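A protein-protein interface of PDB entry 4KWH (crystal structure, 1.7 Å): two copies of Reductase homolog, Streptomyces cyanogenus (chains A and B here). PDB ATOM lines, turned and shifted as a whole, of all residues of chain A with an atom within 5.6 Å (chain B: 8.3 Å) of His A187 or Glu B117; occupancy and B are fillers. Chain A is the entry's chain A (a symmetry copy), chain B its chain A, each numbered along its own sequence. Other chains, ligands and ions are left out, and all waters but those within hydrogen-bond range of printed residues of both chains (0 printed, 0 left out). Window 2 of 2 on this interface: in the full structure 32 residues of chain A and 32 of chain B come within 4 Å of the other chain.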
ATOM      1  N   GLN A 140      -0.919  15.090 -17.154  1.00  0.00           N
ATOM      2  CA  GLN A 140      -2.184  15.674 -16.726  1.00  0.00           C
ATOM      3  C   GLN A 140      -3.047  14.637 -16.004  1.00  0.00           C
ATOM      4  O   GLN A 140      -3.611  14.895 -14.921  1.00  0.00           O
ATOM      5  CB  GLN A 140      -2.923  16.252 -17.928  1.00  0.00           C
ATOM      6  CG  GLN A 140      -4.155  17.046 -17.563  1.00  0.00           C
ATOM      7  CD  GLN A 140      -4.993  17.375 -18.773  1.00  0.00           C
ATOM      8  OE1 GLN A 140      -5.510  16.483 -19.446  1.00  0.00           O
ATOM      9  NE2 GLN A 140      -5.102  18.662 -19.081  1.00  0.00           N
ATOM     10  N   LEU A 143      -1.794  13.301 -12.471  1.00  0.00           N
ATOM     11  CA  LEU A 143      -1.953  14.179 -11.294  1.00  0.00           C
ATOM     12  C   LEU A 143      -3.083  13.752 -10.394  1.00  0.00           C
ATOM     13  O   LEU A 143      -2.972  13.880  -9.185  1.00  0.00           O
ATOM     14  CB  LEU A 143      -2.151  15.641 -11.671  1.00  0.00           C
ATOM     15  CG  LEU A 143      -1.048  16.292 -12.498  1.00  0.00           C
ATOM     16  CD1 LEU A 143      -1.299  17.789 -12.615  1.00  0.00           C
ATOM     17  CD2 LEU A 143       0.315  16.006 -11.886  1.00  0.00           C
ATOM     18  N   HIS A 183       7.652  23.874 -16.101  1.00  0.00           N
ATOM     19  CA  HIS A 183       6.410  24.480 -15.633  1.00  0.00           C
ATOM     20  C   HIS A 183       5.738  23.647 -14.591  1.00  0.00           C
ATOM     21  O   HIS A 183       5.193  24.206 -13.641  1.00  0.00           O
ATOM     22  CB  HIS A 183       5.485  24.794 -16.816  1.00  0.00           C
ATOM     23  CG  HIS A 183       6.119  25.707 -17.821  1.00  0.00           C
ATOM     24  ND1 HIS A 183       6.312  27.010 -17.593  1.00  0.00           N
ATOM     25  CD2 HIS A 183       6.702  25.438 -19.069  1.00  0.00           C
ATOM     26  CE1 HIS A 183       6.952  27.565 -18.651  1.00  0.00           C
ATOM     27  NE2 HIS A 183       7.219  26.597 -19.535  1.00  0.00           N
ATOM     28  N   PHE A 184       5.761  22.323 -14.736  1.00  0.00           N
ATOM     29  CA  PHE A 184       5.089  21.463 -13.748  1.00  0.00           C
ATOM     30  C   PHE A 184       5.869  21.367 -12.437  1.00  0.00           C
ATOM     31  O   PHE A 184       5.258  21.157 -11.376  1.00  0.00           O
ATOM     32  CB  PHE A 184       4.765  20.071 -14.282  1.00  0.00           C
ATOM     33  CG  PHE A 184       3.482  20.002 -15.086  1.00  0.00           C
ATOM     34  CD1 PHE A 184       2.257  19.875 -14.448  1.00  0.00           C
ATOM     35  CD2 PHE A 184       3.501  20.062 -16.463  1.00  0.00           C
ATOM     36  CE1 PHE A 184       1.069  19.812 -15.171  1.00  0.00           C
ATOM     37  CE2 PHE A 184       2.313  19.974 -17.198  1.00  0.00           C
ATOM     38  CZ  PHE A 184       1.101  19.844 -16.549  1.00  0.00           C
ATOM     39  N   SER A 185       7.191  21.558 -12.466  1.00  0.00           N
ATOM     40  CA  SER A 185       7.946  21.548 -11.209  1.00  0.00           C
ATOM     41  C   SER A 185       7.415  22.620 -10.272  1.00  0.00           C
ATOM     42  O   SER A 185       7.233  22.390  -9.071  1.00  0.00           O
ATOM     43  CB  SER A 185       9.450  21.727 -11.416  1.00  0.00           C
ATOM     44  OG  SER A 185       9.730  22.949 -12.040  1.00  0.00           O
ATOM     45  N   ARG A 186       7.135  23.806 -10.811  1.00  0.00           N
ATOM     46  CA  ARG A 186       6.566  24.875 -10.007  1.00  0.00           C
ATOM     47  C   ARG A 186       5.125  24.599  -9.604  1.00  0.00           C
ATOM     48  O   ARG A 186       4.734  24.863  -8.468  1.00  0.00           O
ATOM     49  CB  ARG A 186       6.653  26.224 -10.748  1.00  0.00           C
ATOM     50  CG  ARG A 186       6.064  27.425 -10.004  1.00  0.00           C
ATOM     51  CD  ARG A 186       6.570  28.735 -10.585  1.00  0.00           C
ATOM     52  NE  ARG A 186       7.871  29.106 -10.035  1.00  0.00           N
ATOM     53  CZ  ARG A 186       8.717  29.999 -10.553  1.00  0.00           C
ATOM     54  NH1 ARG A 186       8.443  30.683 -11.676  1.00  0.00           N
ATOM     55  NH2 ARG A 186       9.854  30.243  -9.903  1.00  0.00           N
ATOM     56  N   HIS A 187       4.339  24.063 -10.524  1.00  0.00           N
ATOM     57  CA  HIS A 187       2.940  23.740 -10.231  1.00  0.00           C
ATOM     58  C   HIS A 187       2.816  22.764  -9.079  1.00  0.00           C
ATOM     59  O   HIS A 187       1.891  22.895  -8.244  1.00  0.00           O
ATOM     60  CB  HIS A 187       2.292  23.167 -11.475  1.00  0.00           C
ATOM     61  CG  HIS A 187       0.791  23.054 -11.391  1.00  0.00           C
ATOM     62  ND1 HIS A 187       0.007  24.110 -11.132  1.00  0.00           N
ATOM     63  CD2 HIS A 187      -0.062  21.959 -11.562  1.00  0.00           C
ATOM     64  CE1 HIS A 187      -1.284  23.725 -11.166  1.00  0.00           C
ATOM     65  NE2 HIS A 187      -1.325  22.406 -11.401  1.00  0.00           N
ATOM     66  N   LEU A 188       3.759  21.812  -8.988  1.00  0.00           N
ATOM     67  CA  LEU A 188       3.622  20.654  -8.071  1.00  0.00           C
ATOM     68  C   LEU A 188       4.509  20.732  -6.832  1.00  0.00           C
ATOM     69  O   LEU A 188       4.566  19.788  -6.043  1.00  0.00           O
ATOM     70  CB  LEU A 188       3.892  19.339  -8.827  1.00  0.00           C
ATOM     71  CG  LEU A 188       2.966  19.044 -10.007  1.00  0.00           C
ATOM     72  CD1 LEU A 188       3.403  17.824 -10.800  1.00  0.00           C
ATOM     73  CD2 LEU A 188       1.530  18.873  -9.533  1.00  0.00           C
ATOM     74  N   GLY A 189       5.145  21.874  -6.611  1.00  0.00           N
ATOM     75  CA  GLY A 189       6.069  22.024  -5.491  1.00  0.00           C
ATOM     76  C   GLY A 189       5.438  21.754  -4.138  1.00  0.00           C
ATOM     77  O   GLY A 189       6.035  21.104  -3.287  1.00  0.00           O
ATOM     78  N   SER A 190       4.204  22.220  -3.953  1.00  0.00           N
ATOM     79  CA  SER A 190       3.520  22.058  -2.664  1.00  0.00           C
ATOM     80  C   SER A 190       3.112  20.609  -2.384  1.00  0.00           C
ATOM     81  O   SER A 190       2.825  20.269  -1.237  1.00  0.00           O
ATOM     82  CB  SER A 190       2.303  22.976  -2.594  1.00  0.00           C
ATOM     83  OG  SER A 190       1.280  22.526  -3.456  1.00  0.00           O
ATOM     84  N   GLY B 114      -4.530  29.367 -18.533  1.00  0.00           N
ATOM     85  CA  GLY B 114      -5.546  28.551 -17.886  1.00  0.00           C
ATOM     86  C   GLY B 114      -4.907  27.433 -17.085  1.00  0.00           C
ATOM     87  O   GLY B 114      -3.720  27.118 -17.261  1.00  0.00           O
ATOM     88  N   ALA B 115      -5.686  26.837 -16.197  1.00  0.00           N
ATOM     89  CA  ALA B 115      -5.170  25.783 -15.337  1.00  0.00           C
ATOM     90  C   ALA B 115      -4.708  24.600 -16.183  1.00  0.00           C
ATOM     91  O   ALA B 115      -5.352  24.243 -17.171  1.00  0.00           O
ATOM     92  CB  ALA B 115      -6.207  25.348 -14.323  1.00  0.00           C
ATOM     93  N   PRO B 116      -3.569  24.003 -15.807  1.00  0.00           N
ATOM     94  CA  PRO B 116      -3.052  22.896 -16.654  1.00  0.00           C
ATOM     95  C   PRO B 116      -4.005  21.691 -16.671  1.00  0.00           C
ATOM     96  O   PRO B 116      -4.054  20.965 -17.651  1.00  0.00           O
ATOM     97  CB  PRO B 116      -1.708  22.536 -16.022  1.00  0.00           C
ATOM     98  CG  PRO B 116      -1.534  23.400 -14.833  1.00  0.00           C
ATOM     99  CD  PRO B 116      -2.640  24.393 -14.734  1.00  0.00           C
ATOM    100  N   GLU B 117      -4.810  21.555 -15.622  1.00  0.00           N
ATOM    101  CA  GLU B 117      -5.760  20.451 -15.512  1.00  0.00           C
ATOM    102  C   GLU B 117      -6.904  20.558 -16.529  1.00  0.00           C
ATOM    103  O   GLU B 117      -7.585  19.560 -16.796  1.00  0.00           O
ATOM    104  CB  GLU B 117      -6.319  20.372 -14.080  1.00  0.00           C
ATOM    105  CG  GLU B 117      -5.280  20.061 -12.994  1.00  0.00           C
ATOM    106  CD  GLU B 117      -4.452  21.254 -12.506  1.00  0.00           C
ATOM    107  OE1 GLU B 117      -4.632  22.383 -13.000  1.00  0.00           O
ATOM    108  OE2 GLU B 117      -3.645  21.052 -11.575  1.00  0.00           O
ATOM    109  N   GLU B 118      -7.111  21.755 -17.085  1.00  0.00           N
ATOM    110  CA  GLU B 118      -8.225  22.026 -17.995  1.00  0.00           C
ATOM    111  C   GLU B 118      -7.825  22.087 -19.459  1.00  0.00           C
ATOM    112  O   GLU B 118      -8.680  22.283 -20.341  1.00  0.00           O
ATOM    113  CB  GLU B 118      -8.893  23.340 -17.629  1.00  0.00           C
ATOM    114  CG  GLU B 118      -9.470  23.331 -16.230  1.00  0.00           C
ATOM    115  CD  GLU B 118     -10.207  24.606 -15.899  1.00  0.00           C
ATOM    116  OE1 GLU B 118     -10.236  25.535 -16.748  1.00  0.00           O
ATOM    117  OE2 GLU B 118     -10.757  24.676 -14.780  1.00  0.00           O
ATOM    118  N   VAL B 119      -6.537  21.949 -19.740  1.00  0.00           N
ATOM    119  CA  VAL B 119      -6.086  21.915 -21.125  1.00  0.00           C
ATOM    120  C   VAL B 119      -6.662  20.697 -21.853  1.00  0.00           C
ATOM    121  O   VAL B 119      -6.547  19.571 -21.375  1.00  0.00           O
ATOM    122  CB  VAL B 119      -4.554  21.884 -21.240  1.00  0.00           C
ATOM    123  CG1 VAL B 119      -4.145  21.716 -22.697  1.00  0.00           C
ATOM    124  CG2 VAL B 119      -3.922  23.143 -20.658  1.00  0.00           C
ATOM    125  N   THR B 120      -7.291  20.936 -23.000  1.00  0.00           N
ATOM    126  CA  THR B 120      -7.814  19.873 -23.851  1.00  0.00           C
ATOM    127  C   THR B 120      -6.838  19.516 -24.991  1.00  0.00           C
ATOM    128  O   THR B 120      -6.002  20.338 -25.377  1.00  0.00           O
ATOM    129  CB  THR B 120      -9.165  20.271 -24.477  1.00  0.00           C
ATOM    130  OG1 THR B 120      -8.990  21.321 -25.431  1.00  0.00           O
ATOM    131  CG2 THR B 120     -10.170  20.725 -23.391  1.00  0.00           C
ATOM    132  N   MET B 123      -7.033  22.280 -27.623  1.00  0.00           N
ATOM    133  CA  MET B 123      -6.236  23.442 -27.237  1.00  0.00           C
ATOM    134  C   MET B 123      -4.754  23.208 -27.497  1.00  0.00           C
ATOM    135  O   MET B 123      -4.046  24.097 -28.005  1.00  0.00           O
ATOM    136  CB  MET B 123      -6.475  23.759 -25.761  1.00  0.00           C
ATOM    137  CG  MET B 123      -7.867  24.300 -25.493  1.00  0.00           C
ATOM    138  SD  MET B 123      -8.303  24.210 -23.741  1.00  0.00           S
ATOM    139  CE  MET B 123      -7.142  25.358 -23.029  1.00  0.00           C
ATOM    140  N   ALA B 163       9.150  29.415 -15.126  1.00  0.00           N
ATOM    141  CA  ALA B 163       8.093  28.441 -14.862  1.00  0.00           C
ATOM    142  C   ALA B 163       6.785  29.173 -14.645  1.00  0.00           C
ATOM    143  O   ALA B 163       6.694  30.062 -13.785  1.00  0.00           O
ATOM    144  CB  ALA B 163       8.450  27.585 -13.652  1.00  0.00           C
ATOM    145  N   SER B 164       5.785  28.812 -15.447  1.00  0.00           N
ATOM    146  CA  SER B 164       4.515  29.517 -15.547  1.00  0.00           C
ATOM    147  C   SER B 164       3.402  28.487 -15.791  1.00  0.00           C
ATOM    148  O   SER B 164       2.976  28.282 -16.921  1.00  0.00           O
ATOM    149  CB  SER B 164       4.569  30.529 -16.694  1.00  0.00           C
ATOM    150  OG  SER B 164       5.660  31.439 -16.541  1.00  0.00           O
ATOM    151  N   PRO B 165       2.927  27.822 -14.721  1.00  0.00           N
ATOM    152  CA  PRO B 165       2.019  26.678 -14.918  1.00  0.00           C
ATOM    153  C   PRO B 165       0.763  26.968 -15.749  1.00  0.00           C
ATOM    154  O   PRO B 165       0.305  26.083 -16.488  1.00  0.00           O
ATOM    155  CB  PRO B 165       1.661  26.275 -13.492  1.00  0.00           C
ATOM    156  CG  PRO B 165       2.820  26.706 -12.665  1.00  0.00           C
ATOM    157  CD  PRO B 165       3.385  27.929 -13.324  1.00  0.00           C
ATOM    158  N   ASP B 166       0.243  28.199 -15.694  1.00  0.00           N
ATOM    159  CA  ASP B 166      -0.971  28.530 -16.438  1.00  0.00           C
ATOM    160  C   ASP B 166      -0.701  28.746 -17.916  1.00  0.00           C
ATOM    161  O   ASP B 166      -1.638  28.954 -18.695  1.00  0.00           O
ATOM    162  CB  ASP B 166      -1.675  29.742 -15.820  1.00  0.00           C
ATOM    163  CG  ASP B 166      -2.429  29.395 -14.557  1.00  0.00           C
ATOM    164  OD1 ASP B 166      -2.531  28.192 -14.202  1.00  0.00           O
ATOM    165  OD2 ASP B 166      -2.944  30.331 -13.912  1.00  0.00           O
ATOM    166  N   VAL B 168       1.742  26.457 -19.583  1.00  0.00           N
ATOM    167  CA  VAL B 168       2.639  25.353 -19.947  1.00  0.00           C
ATOM    168  C   VAL B 168       2.520  24.941 -21.422  1.00  0.00           C
ATOM    169  O   VAL B 168       3.518  24.644 -22.053  1.00  0.00           O
ATOM    170  CB  VAL B 168       2.457  24.122 -19.037  1.00  0.00           C
ATOM    171  CG1 VAL B 168       1.024  23.639 -19.047  1.00  0.00           C
ATOM    172  CG2 VAL B 168       3.427  23.008 -19.445  1.00  0.00           C
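The backbone carbonyl oxygen (O) of Pro B116 is in hydrogen-bond range of the side-chain amide nitrogen (NE2) of Gln A140, at 2.9 Å. O of Glu B117 sits at hydrogen-bond distance from NE2 of Gln A140 (3.5 Å). NE2 of His A187 is in hydrogen-bond range of OE2 of Glu B117. The side-chain amide nitrogen (NE2) of Gln A140 is in hydrogen-bond range of the backbone carbonyl oxygen (O) of Val B119. O of Ala B163 sits at hydrogen-bond distance from NH1 of Arg A186, at 2.8 Å. The backbone NH (N) of Ser B164 lies within hydrogen-bond range of a ring nitrogen (ND1) of His A183 (2.9 Å).
CA of Ala B163 touches ND1 of His A183 (3.6 Å). His A183 touches Pro B165. Val B168 touches His A183. Pro B116 touches Phe A184 (CB to CZ, 3.9 Å). Val B168 touches Phe A184 (CG2 to CE2, 3.9 Å). Pro B116 touches His A187. His A187 touches Pro B165 (ND1 to CB, 3.6 Å).
Leu A143 touches none of the printed residues of chain B. Printed residues of chain B within 4 Å of Arg A186: Ala B163 (2.8 Å). Of chain B, only Pro B116, Glu B117 and Pro B165 come within 4 Å of His A187. Ala B115 touches none of the printed residues of chain A. Of the printed residues of chain A, Pro B116 touches Gln A140, Phe A184 and His A187. Of chain A, only Gln A140 and His A187 come within 4 Å of Glu B117. Of the printed residues of chain A, Val B119 touches Gln A140. Of the printed residues of chain A, Ser B164 touches His A183. The nearest printed residue of chain A that does not touch Ala B163 is Ser A185 (5.1 Å).
Of the 13 printed residues of chain B, 7 touch a printed residue of chain A. Printed residues of chain B that touch a printed residue of chain A: Pro B116, Glu B117, Val B119, Ala B163, Ser B164, Pro B165 and Val B168. Hydrophobic or aromatic side chains of chain A that line the printed part of chain B: His A183, Phe A184 and His A187. Among the printed residues, 13 pairs touch across the chains. Among the printed residues, no Asp or Glu carboxylate lies within 4 Å of a Lys or Arg side-chain nitrogen of the other chain.
No position is printed for both chains.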
